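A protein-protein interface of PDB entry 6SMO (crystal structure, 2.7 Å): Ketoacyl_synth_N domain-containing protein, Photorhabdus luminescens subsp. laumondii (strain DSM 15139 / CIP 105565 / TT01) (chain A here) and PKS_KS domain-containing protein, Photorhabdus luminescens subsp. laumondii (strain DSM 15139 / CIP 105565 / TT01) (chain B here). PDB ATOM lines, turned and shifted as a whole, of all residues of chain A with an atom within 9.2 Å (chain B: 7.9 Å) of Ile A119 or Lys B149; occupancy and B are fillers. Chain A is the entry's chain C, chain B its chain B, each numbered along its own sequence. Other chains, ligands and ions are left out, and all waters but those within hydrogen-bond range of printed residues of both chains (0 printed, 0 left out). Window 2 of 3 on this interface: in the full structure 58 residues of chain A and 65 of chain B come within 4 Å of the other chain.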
ATOM      1  N   ASP A 112      16.742 -10.913  13.323  1.00  0.00           N
ATOM      2  CA  ASP A 112      17.990 -11.684  13.063  1.00  0.00           C
ATOM      3  C   ASP A 112      18.129 -12.806  14.101  1.00  0.00           C
ATOM      4  O   ASP A 112      18.642 -13.885  13.738  1.00  0.00           O
ATOM      5  CB  ASP A 112      19.219 -10.770  13.064  1.00  0.00           C
ATOM      6  CG  ASP A 112      19.253  -9.767  11.923  1.00  0.00           C
ATOM      7  OD1 ASP A 112      18.307  -9.767  11.109  1.00  0.00           O
ATOM      8  OD2 ASP A 112      20.226  -8.988  11.859  1.00  0.00           O
ATOM      9  N   GLU A 113      17.680 -12.559  15.335  1.00  0.00           N
ATOM     10  CA  GLU A 113      17.777 -13.510  16.475  1.00  0.00           C
ATOM     11  C   GLU A 113      16.782 -14.666  16.287  1.00  0.00           C
ATOM     12  O   GLU A 113      17.137 -15.801  16.661  1.00  0.00           O
ATOM     13  CB  GLU A 113      17.567 -12.768  17.797  1.00  0.00           C
ATOM     14  CG  GLU A 113      18.757 -11.913  18.197  1.00  0.00           C
ATOM     15  CD  GLU A 113      18.600 -11.179  19.518  1.00  0.00           C
ATOM     16  OE1 GLU A 113      19.390 -11.456  20.444  1.00  0.00           O
ATOM     17  OE2 GLU A 113      17.695 -10.327  19.616  1.00  0.00           O
ATOM     18  N   VAL A 114      15.596 -14.401  15.722  1.00  0.00           N
ATOM     19  CA  VAL A 114      14.550 -15.438  15.463  1.00  0.00           C
ATOM     20  C   VAL A 114      15.037 -16.363  14.340  1.00  0.00           C
ATOM     21  O   VAL A 114      14.783 -17.577  14.434  1.00  0.00           O
ATOM     22  CB  VAL A 114      13.176 -14.820  15.131  1.00  0.00           C
ATOM     23  CG1 VAL A 114      12.130 -15.886  14.831  1.00  0.00           C
ATOM     24  CG2 VAL A 114      12.683 -13.906  16.243  1.00  0.00           C
ATOM     25  N   LYS A 115      15.710 -15.813  13.323  1.00  0.00           N
ATOM     26  CA  LYS A 115      16.247 -16.576  12.161  1.00  0.00           C
ATOM     27  C   LYS A 115      17.449 -17.420  12.605  1.00  0.00           C
ATOM     28  O   LYS A 115      17.532 -18.590  12.182  1.00  0.00           O
ATOM     29  CB  LYS A 115      16.636 -15.631  11.020  1.00  0.00           C
ATOM     30  CG  LYS A 115      15.481 -14.863  10.393  1.00  0.00           C
ATOM     31  CD  LYS A 115      15.756 -14.380   8.984  1.00  0.00           C
ATOM     32  CE  LYS A 115      16.867 -13.355   8.902  1.00  0.00           C
ATOM     33  NZ  LYS A 115      17.096 -12.912   7.506  1.00  0.00           N
ATOM     34  N   ALA A 116      18.337 -16.847  13.428  1.00  0.00           N
ATOM     35  CA  ALA A 116      19.604 -17.466  13.892  1.00  0.00           C
ATOM     36  C   ALA A 116      19.323 -18.627  14.857  1.00  0.00           C
ATOM     37  O   ALA A 116      20.185 -19.523  14.960  1.00  0.00           O
ATOM     38  CB  ALA A 116      20.480 -16.419  14.536  1.00  0.00           C
ATOM     39  N   LEU A 117      18.171 -18.606  15.538  1.00  0.00           N
ATOM     40  CA  LEU A 117      17.731 -19.650  16.507  1.00  0.00           C
ATOM     41  C   LEU A 117      17.557 -20.995  15.785  1.00  0.00           C
ATOM     42  O   LEU A 117      17.862 -22.032  16.404  1.00  0.00           O
ATOM     43  CB  LEU A 117      16.428 -19.185  17.171  1.00  0.00           C
ATOM     44  CG  LEU A 117      15.701 -20.209  18.047  1.00  0.00           C
ATOM     45  CD1 LEU A 117      16.130 -20.096  19.503  1.00  0.00           C
ATOM     46  CD2 LEU A 117      14.194 -20.040  17.934  1.00  0.00           C
ATOM     47  N   HIS A 118      17.112 -20.974  14.523  1.00  0.00           N
ATOM     48  CA  HIS A 118      16.759 -22.177  13.718  1.00  0.00           C
ATOM     49  C   HIS A 118      17.973 -22.707  12.942  1.00  0.00           C
ATOM     50  O   HIS A 118      17.827 -23.762  12.292  1.00  0.00           O
ATOM     51  CB  HIS A 118      15.573 -21.862  12.798  1.00  0.00           C
ATOM     52  CG  HIS A 118      14.294 -21.701  13.545  1.00  0.00           C
ATOM     53  ND1 HIS A 118      13.322 -22.681  13.567  1.00  0.00           N
ATOM     54  CD2 HIS A 118      13.840 -20.699  14.327  1.00  0.00           C
ATOM     55  CE1 HIS A 118      12.316 -22.280  14.317  1.00  0.00           C
ATOM     56  NE2 HIS A 118      12.610 -21.067  14.796  1.00  0.00           N
ATOM     57  N   ILE A 119      19.117 -22.015  13.009  1.00  0.00           N
ATOM     58  CA  ILE A 119      20.398 -22.429  12.360  1.00  0.00           C
ATOM     59  C   ILE A 119      21.408 -22.796  13.453  1.00  0.00           C
ATOM     60  O   ILE A 119      21.872 -23.955  13.463  1.00  0.00           O
ATOM     61  CB  ILE A 119      20.932 -21.318  11.432  1.00  0.00           C
ATOM     62  CG1 ILE A 119      19.916 -20.957  10.345  1.00  0.00           C
ATOM     63  CG2 ILE A 119      22.277 -21.710  10.835  1.00  0.00           C
ATOM     64  CD1 ILE A 119      20.188 -19.640   9.659  1.00  0.00           C
ATOM     65  N   GLU A 120      21.734 -21.839  14.329  1.00  0.00           N
ATOM     66  CA  GLU A 120      22.765 -21.978  15.393  1.00  0.00           C
ATOM     67  C   GLU A 120      22.174 -22.725  16.596  1.00  0.00           C
ATOM     68  O   GLU A 120      22.797 -23.709  17.040  1.00  0.00           O
ATOM     69  CB  GLU A 120      23.279 -20.603  15.826  1.00  0.00           C
ATOM     70  CG  GLU A 120      23.939 -19.818  14.706  1.00  0.00           C
ATOM     71  CD  GLU A 120      24.311 -18.392  15.076  1.00  0.00           C
ATOM     72  OE1 GLU A 120      24.060 -17.486  14.255  1.00  0.00           O
ATOM     73  OE2 GLU A 120      24.851 -18.190  16.182  1.00  0.00           O
ATOM     74  N   GLY A 121      21.022 -22.264  17.093  1.00  0.00           N
ATOM     75  CA  GLY A 121      20.380 -22.754  18.330  1.00  0.00           C
ATOM     76  C   GLY A 121      20.158 -21.618  19.313  1.00  0.00           C
ATOM     77  O   GLY A 121      19.931 -20.484  18.855  1.00  0.00           O
ATOM     78  N   ILE A 122      20.236 -21.905  20.617  1.00  0.00           N
ATOM     79  CA  ILE A 122      20.019 -20.913  21.716  1.00  0.00           C
ATOM     80  C   ILE A 122      21.065 -19.792  21.625  1.00  0.00           C
ATOM     81  O   ILE A 122      20.713 -18.643  21.961  1.00  0.00           O
ATOM     82  CB  ILE A 122      20.026 -21.580  23.108  1.00  0.00           C
ATOM     83  CG1 ILE A 122      19.690 -20.563  24.201  1.00  0.00           C
ATOM     84  CG2 ILE A 122      21.346 -22.289  23.388  1.00  0.00           C
ATOM     85  CD1 ILE A 122      19.382 -21.179  25.538  1.00  0.00           C
ATOM     86  N   LYS A 123      22.294 -20.113  21.203  1.00  0.00           N
ATOM     87  CA  LYS A 123      23.409 -19.139  21.020  1.00  0.00           C
ATOM     88  C   LYS A 123      22.964 -18.007  20.084  1.00  0.00           C
ATOM     89  O   LYS A 123      23.480 -16.882  20.237  1.00  0.00           O
ATOM     90  CB  LYS A 123      24.649 -19.835  20.450  1.00  0.00           C
ATOM     91  CG  LYS A 123      25.374 -20.769  21.410  1.00  0.00           C
ATOM     92  CD  LYS A 123      26.617 -21.400  20.815  1.00  0.00           C
ATOM     93  CE  LYS A 123      27.457 -22.138  21.836  1.00  0.00           C
ATOM     94  NZ  LYS A 123      26.772 -23.350  22.344  1.00  0.00           N
ATOM     95  N   GLY A 124      22.047 -18.306  19.156  1.00  0.00           N
ATOM     96  CA  GLY A 124      21.529 -17.379  18.132  1.00  0.00           C
ATOM     97  C   GLY A 124      20.844 -16.157  18.724  1.00  0.00           C
ATOM     98  O   GLY A 124      21.169 -15.040  18.270  1.00  0.00           O
ATOM     99  N   MET A 125      19.927 -16.340  19.683  1.00  0.00           N
ATOM    100  CA  MET A 125      19.122 -15.224  20.255  1.00  0.00           C
ATOM    101  C   MET A 125      19.523 -14.957  21.712  1.00  0.00           C
ATOM    102  O   MET A 125      19.720 -15.926  22.473  1.00  0.00           O
ATOM    103  CB  MET A 125      17.613 -15.477  20.142  1.00  0.00           C
ATOM    104  CG  MET A 125      17.050 -16.601  20.993  1.00  0.00           C
ATOM    105  SD  MET A 125      15.238 -16.493  21.103  1.00  0.00           S
ATOM    106  CE  MET A 125      14.803 -16.032  19.426  1.00  0.00           C
ATOM    107  N   ARG B  67      16.728 -30.431  19.042  1.00  0.00           N
ATOM    108  CA  ARG B  67      16.795 -29.584  17.817  1.00  0.00           C
ATOM    109  C   ARG B  67      17.496 -28.254  18.131  1.00  0.00           C
ATOM    110  O   ARG B  67      18.495 -27.946  17.449  1.00  0.00           O
ATOM    111  CB  ARG B  67      15.387 -29.368  17.246  1.00  0.00           C
ATOM    112  CG  ARG B  67      15.258 -28.217  16.258  1.00  0.00           C
ATOM    113  CD  ARG B  67      16.056 -28.396  14.980  1.00  0.00           C
ATOM    114  NE  ARG B  67      15.913 -27.240  14.101  1.00  0.00           N
ATOM    115  CZ  ARG B  67      16.413 -27.144  12.870  1.00  0.00           C
ATOM    116  NH1 ARG B  67      16.217 -26.041  12.167  1.00  0.00           N
ATOM    117  NH2 ARG B  67      17.103 -28.142  12.343  1.00  0.00           N
ATOM    118  N   PHE B  68      16.990 -27.501  19.113  1.00  0.00           N
ATOM    119  CA  PHE B  68      17.377 -26.090  19.393  1.00  0.00           C
ATOM    120  C   PHE B  68      18.440 -26.012  20.497  1.00  0.00           C
ATOM    121  O   PHE B  68      19.255 -25.068  20.460  1.00  0.00           O
ATOM    122  CB  PHE B  68      16.140 -25.265  19.753  1.00  0.00           C
ATOM    123  CG  PHE B  68      15.149 -25.128  18.624  1.00  0.00           C
ATOM    124  CD1 PHE B  68      15.403 -24.274  17.562  1.00  0.00           C
ATOM    125  CD2 PHE B  68      13.973 -25.862  18.615  1.00  0.00           C
ATOM    126  CE1 PHE B  68      14.497 -24.151  16.519  1.00  0.00           C
ATOM    127  CE2 PHE B  68      13.069 -25.739  17.571  1.00  0.00           C
ATOM    128  CZ  PHE B  68      13.333 -24.884  16.525  1.00  0.00           C
ATOM    129  N   LEU B 141       7.892 -15.969   8.838  1.00  0.00           N
ATOM    130  CA  LEU B 141       9.231 -15.330   8.692  1.00  0.00           C
ATOM    131  C   LEU B 141      10.252 -16.345   8.159  1.00  0.00           C
ATOM    132  O   LEU B 141      11.046 -15.967   7.277  1.00  0.00           O
ATOM    133  CB  LEU B 141       9.662 -14.768  10.051  1.00  0.00           C
ATOM    134  CG  LEU B 141      11.102 -14.261  10.155  1.00  0.00           C
ATOM    135  CD1 LEU B 141      11.362 -13.120   9.182  1.00  0.00           C
ATOM    136  CD2 LEU B 141      11.414 -13.823  11.577  1.00  0.00           C
ATOM    137  N   LEU B 142      10.238 -17.575   8.682  1.00  0.00           N
ATOM    138  CA  LEU B 142      11.227 -18.638   8.350  1.00  0.00           C
ATOM    139  C   LEU B 142      10.892 -19.271   6.993  1.00  0.00           C
ATOM    140  O   LEU B 142      11.836 -19.710   6.304  1.00  0.00           O
ATOM    141  CB  LEU B 142      11.236 -19.684   9.469  1.00  0.00           C
ATOM    142  CG  LEU B 142      11.858 -19.217  10.783  1.00  0.00           C
ATOM    143  CD1 LEU B 142      11.493 -20.157  11.919  1.00  0.00           C
ATOM    144  CD2 LEU B 142      13.368 -19.091  10.657  1.00  0.00           C
ATOM    145  N   ILE B 144       9.425 -17.623   4.340  1.00  0.00           N
ATOM    146  CA  ILE B 144       9.732 -16.602   3.288  1.00  0.00           C
ATOM    147  C   ILE B 144      11.252 -16.423   3.147  1.00  0.00           C
ATOM    148  O   ILE B 144      11.676 -15.941   2.078  1.00  0.00           O
ATOM    149  CB  ILE B 144       9.014 -15.261   3.567  1.00  0.00           C
ATOM    150  CG1 ILE B 144       9.447 -14.621   4.891  1.00  0.00           C
ATOM    151  CG2 ILE B 144       7.505 -15.446   3.480  1.00  0.00           C
ATOM    152  CD1 ILE B 144       8.753 -13.314   5.215  1.00  0.00           C
ATOM    153  N   THR B 145      12.036 -16.789   4.170  1.00  0.00           N
ATOM    154  CA  THR B 145      13.523 -16.685   4.180  1.00  0.00           C
ATOM    155  C   THR B 145      14.165 -18.063   3.961  1.00  0.00           C
ATOM    156  O   THR B 145      15.412 -18.125   3.959  1.00  0.00           O
ATOM    157  CB  THR B 145      14.025 -16.050   5.485  1.00  0.00           C
ATOM    158  OG1 THR B 145      13.486 -16.790   6.581  1.00  0.00           O
ATOM    159  CG2 THR B 145      13.639 -14.593   5.616  1.00  0.00           C
ATOM    160  N   LYS B 146      13.355 -19.113   3.773  1.00  0.00           N
ATOM    161  CA  LYS B 146      13.801 -20.523   3.578  1.00  0.00           C
ATOM    162  C   LYS B 146      14.695 -20.945   4.753  1.00  0.00           C
ATOM    163  O   LYS B 146      15.928 -21.014   4.569  1.00  0.00           O
ATOM    164  CB  LYS B 146      14.516 -20.689   2.231  1.00  0.00           C
ATOM    165  CG  LYS B 146      13.614 -20.639   1.005  1.00  0.00           C
ATOM    166  CD  LYS B 146      14.302 -21.084  -0.270  1.00  0.00           C
ATOM    167  CE  LYS B 146      13.349 -21.273  -1.432  1.00  0.00           C
ATOM    168  NZ  LYS B 146      12.900 -19.976  -1.993  1.00  0.00           N
ATOM    169  N   GLY B 147      14.085 -21.205   5.914  1.00  0.00           N
ATOM    170  CA  GLY B 147      14.761 -21.692   7.133  1.00  0.00           C
ATOM    171  C   GLY B 147      15.667 -20.643   7.760  1.00  0.00           C
ATOM    172  O   GLY B 147      16.590 -21.038   8.502  1.00  0.00           O
ATOM    173  N   GLY B 148      15.422 -19.358   7.480  1.00  0.00           N
ATOM    174  CA  GLY B 148      16.149 -18.214   8.064  1.00  0.00           C
ATOM    175  C   GLY B 148      17.565 -18.069   7.528  1.00  0.00           C
ATOM    176  O   GLY B 148      18.356 -17.351   8.172  1.00  0.00           O
ATOM    177  N   LYS B 149      17.879 -18.703   6.391  1.00  0.00           N
ATOM    178  CA  LYS B 149      19.238 -18.713   5.777  1.00  0.00           C
ATOM    179  C   LYS B 149      19.413 -17.475   4.889  1.00  0.00           C
ATOM    180  O   LYS B 149      20.439 -16.783   5.042  1.00  0.00           O
ATOM    181  CB  LYS B 149      19.462 -19.995   4.968  1.00  0.00           C
ATOM    182  CG  LYS B 149      19.905 -21.207   5.777  1.00  0.00           C
ATOM    183  CD  LYS B 149      21.373 -21.179   6.159  1.00  0.00           C
ATOM    184  CE  LYS B 149      21.781 -22.326   7.060  1.00  0.00           C
ATOM    185  NZ  LYS B 149      21.715 -23.632   6.361  1.00  0.00           N
ATOM    186  N   GLU B 150      18.448 -17.217   4.000  1.00  0.00           N
ATOM    187  CA  GLU B 150      18.504 -16.149   2.963  1.00  0.00           C
ATOM    188  C   GLU B 150      17.730 -14.912   3.437  1.00  0.00           C
ATOM    189  O   GLU B 150      17.186 -14.943   4.560  1.00  0.00           O
ATOM    190  CB  GLU B 150      17.921 -16.672   1.648  1.00  0.00           C
ATOM    191  CG  GLU B 150      18.639 -17.895   1.106  1.00  0.00           C
ATOM    192  CD  GLU B 150      18.088 -18.426  -0.208  1.00  0.00           C
ATOM    193  OE1 GLU B 150      18.885 -18.947  -1.011  1.00  0.00           O
ATOM    194  OE2 GLU B 150      16.863 -18.323  -0.421  1.00  0.00           O
ATOM    195  N   ASN B 151      17.696 -13.867   2.603  1.00  0.00           N
ATOM    196  CA  ASN B 151      16.854 -12.653   2.787  1.00  0.00           C
ATOM    197  C   ASN B 151      15.388 -13.024   2.532  1.00  0.00           C
ATOM    198  O   ASN B 151      15.133 -14.164   2.096  1.00  0.00           O
ATOM    199  CB  ASN B 151      17.297 -11.506   1.873  1.00  0.00           C
ATOM    200  CG  ASN B 151      18.627 -10.904   2.273  1.00  0.00           C
ATOM    201  OD1 ASN B 151      19.394 -11.511   3.019  1.00  0.00           O
ATOM    202  ND2 ASN B 151      18.910  -9.708   1.783  1.00  0.00           N
ATOM    203  N   ILE B 152      14.465 -12.094   2.793  1.00  0.00           N
ATOM    204  CA  ILE B 152      12.994 -12.295   2.628  1.00  0.00           C
ATOM    205  C   ILE B 152      12.651 -12.277   1.133  1.00  0.00           C
ATOM    206  O   ILE B 152      13.016 -11.299   0.452  1.00  0.00           O
ATOM    207  CB  ILE B 152      12.199 -11.236   3.422  1.00  0.00           C
ATOM    208  CG1 ILE B 152      12.288 -11.493   4.929  1.00  0.00           C
ATOM    209  CG2 ILE B 152      10.754 -11.166   2.949  1.00  0.00           C
ATOM    210  CD1 ILE B 152      11.964 -10.291   5.780  1.00  0.00           C
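CD2 of Leu B141 touches CG1 of Val A114, at 3.9 Å.
Lys A115 touches Thr B145 (CD to CG2, 3.98 Å).
Lys A115 touches Gly B148 (CB to O, 3.7 Å).
Glu B150 touches Lys A115 (O to NZ, 3.6 Å).
Phe B68 touches Leu A117 (CD1 to O, 3.5 Å).
CE1 of Phe B68 touches ND1 of His A118, 3.5 Å away.
NE2 of His A118 touches CD1 of Leu B142, at 3.2 Å.
CG1 of Ile A119 touches O of Gly B147 (3.8 Å).
CE of Lys B149 touches CG2 of Ile A119, 3.9 Å away.
O of Phe B68 touches CA of Gly A121, at 3.3 Å.
Of the printed residues of chain B, His A118 touches Arg B67 (2.8 Å), Phe B68 (3.5 Å) and Leu B142 (3.2 Å).
Of chain B, only Gly B147 (3.8 Å), Gly B148 (3.3 Å) and Lys B149 (3.9 Å) come within 4 Å of Ile A119.
Of the printed residues of chain B, Ile A122 touches Phe B68.
Of the printed residues of chain A, Arg B67 touches His A118 (2.8 Å).
Of the printed residues of chain A, Leu B141 touches Val A114 (3.9 Å).
Of the printed residues of chain A, Thr B145 touches Lys A115 (3.98 Å).
Lys B146 touches none of the printed residues of chain A.
Gly B147 touches just one residue of chain A: Ile A119 (3.8 Å).
Lys B149 touches just one residue of chain A: Ile A119.
Ile B152 touches none of the printed residues of chain A.
The nearest residue of chain B that does not touch Ile A119 is Arg B67 (5.0 Å).
NH1 of Arg B67 lies within hydrogen-bond range of O of His A118, at 2.8 Å.
N of Ile A122 is in hydrogen-bond range of O of Phe B68 (3.3 Å).
The backbone carbonyl oxygen of Leu B141 sits at hydrogen-bond distance from the side-chain hydroxyl of Thr B145, at 2.7 Å.
O of Leu B142 lies within hydrogen-bond range of OG1 of Thr B145 (3.4 Å).
N of Gly B147 sits at hydrogen-bond distance from O of Leu B142 (2.7 Å).
OG1 of Thr B145 lies within hydrogen-bond range of N of Gly B148, 3.3 Å away.
The backbone carbonyl oxygen (O) of Thr B145 sits at hydrogen-bond distance from the backbone NH (N) of Glu B150 (3.2 Å).
Printed residues of chain B that touch a printed residue of chain A: Arg B67, Phe B68, Leu B141, Leu B142, Thr B145, Gly B147, Gly B148, Lys B149 and Glu B150.
Hydrophobic or aromatic side chains of chain B that line the printed part of chain A: Phe B68, Leu B141 and Leu B142.
Of the 14 printed residues of chain A, 7 touch a printed residue of chain B.
Printed residues of chain A that touch a printed residue of chain B: Val A114, Lys A115, Leu A117, His A118, Ile A119, Gly A121 and Ile A122.
Hydrophobic or aromatic side chains of chain A that line the printed part of chain B: Val A114, His A118 and Ile A119.
Among the printed residues, 13 pairs touch across the chains.
Among the printed residues, no Asp or Glu carboxylate lies within 4 Å of a Lys or Arg side-chain nitrogen of the other chain.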
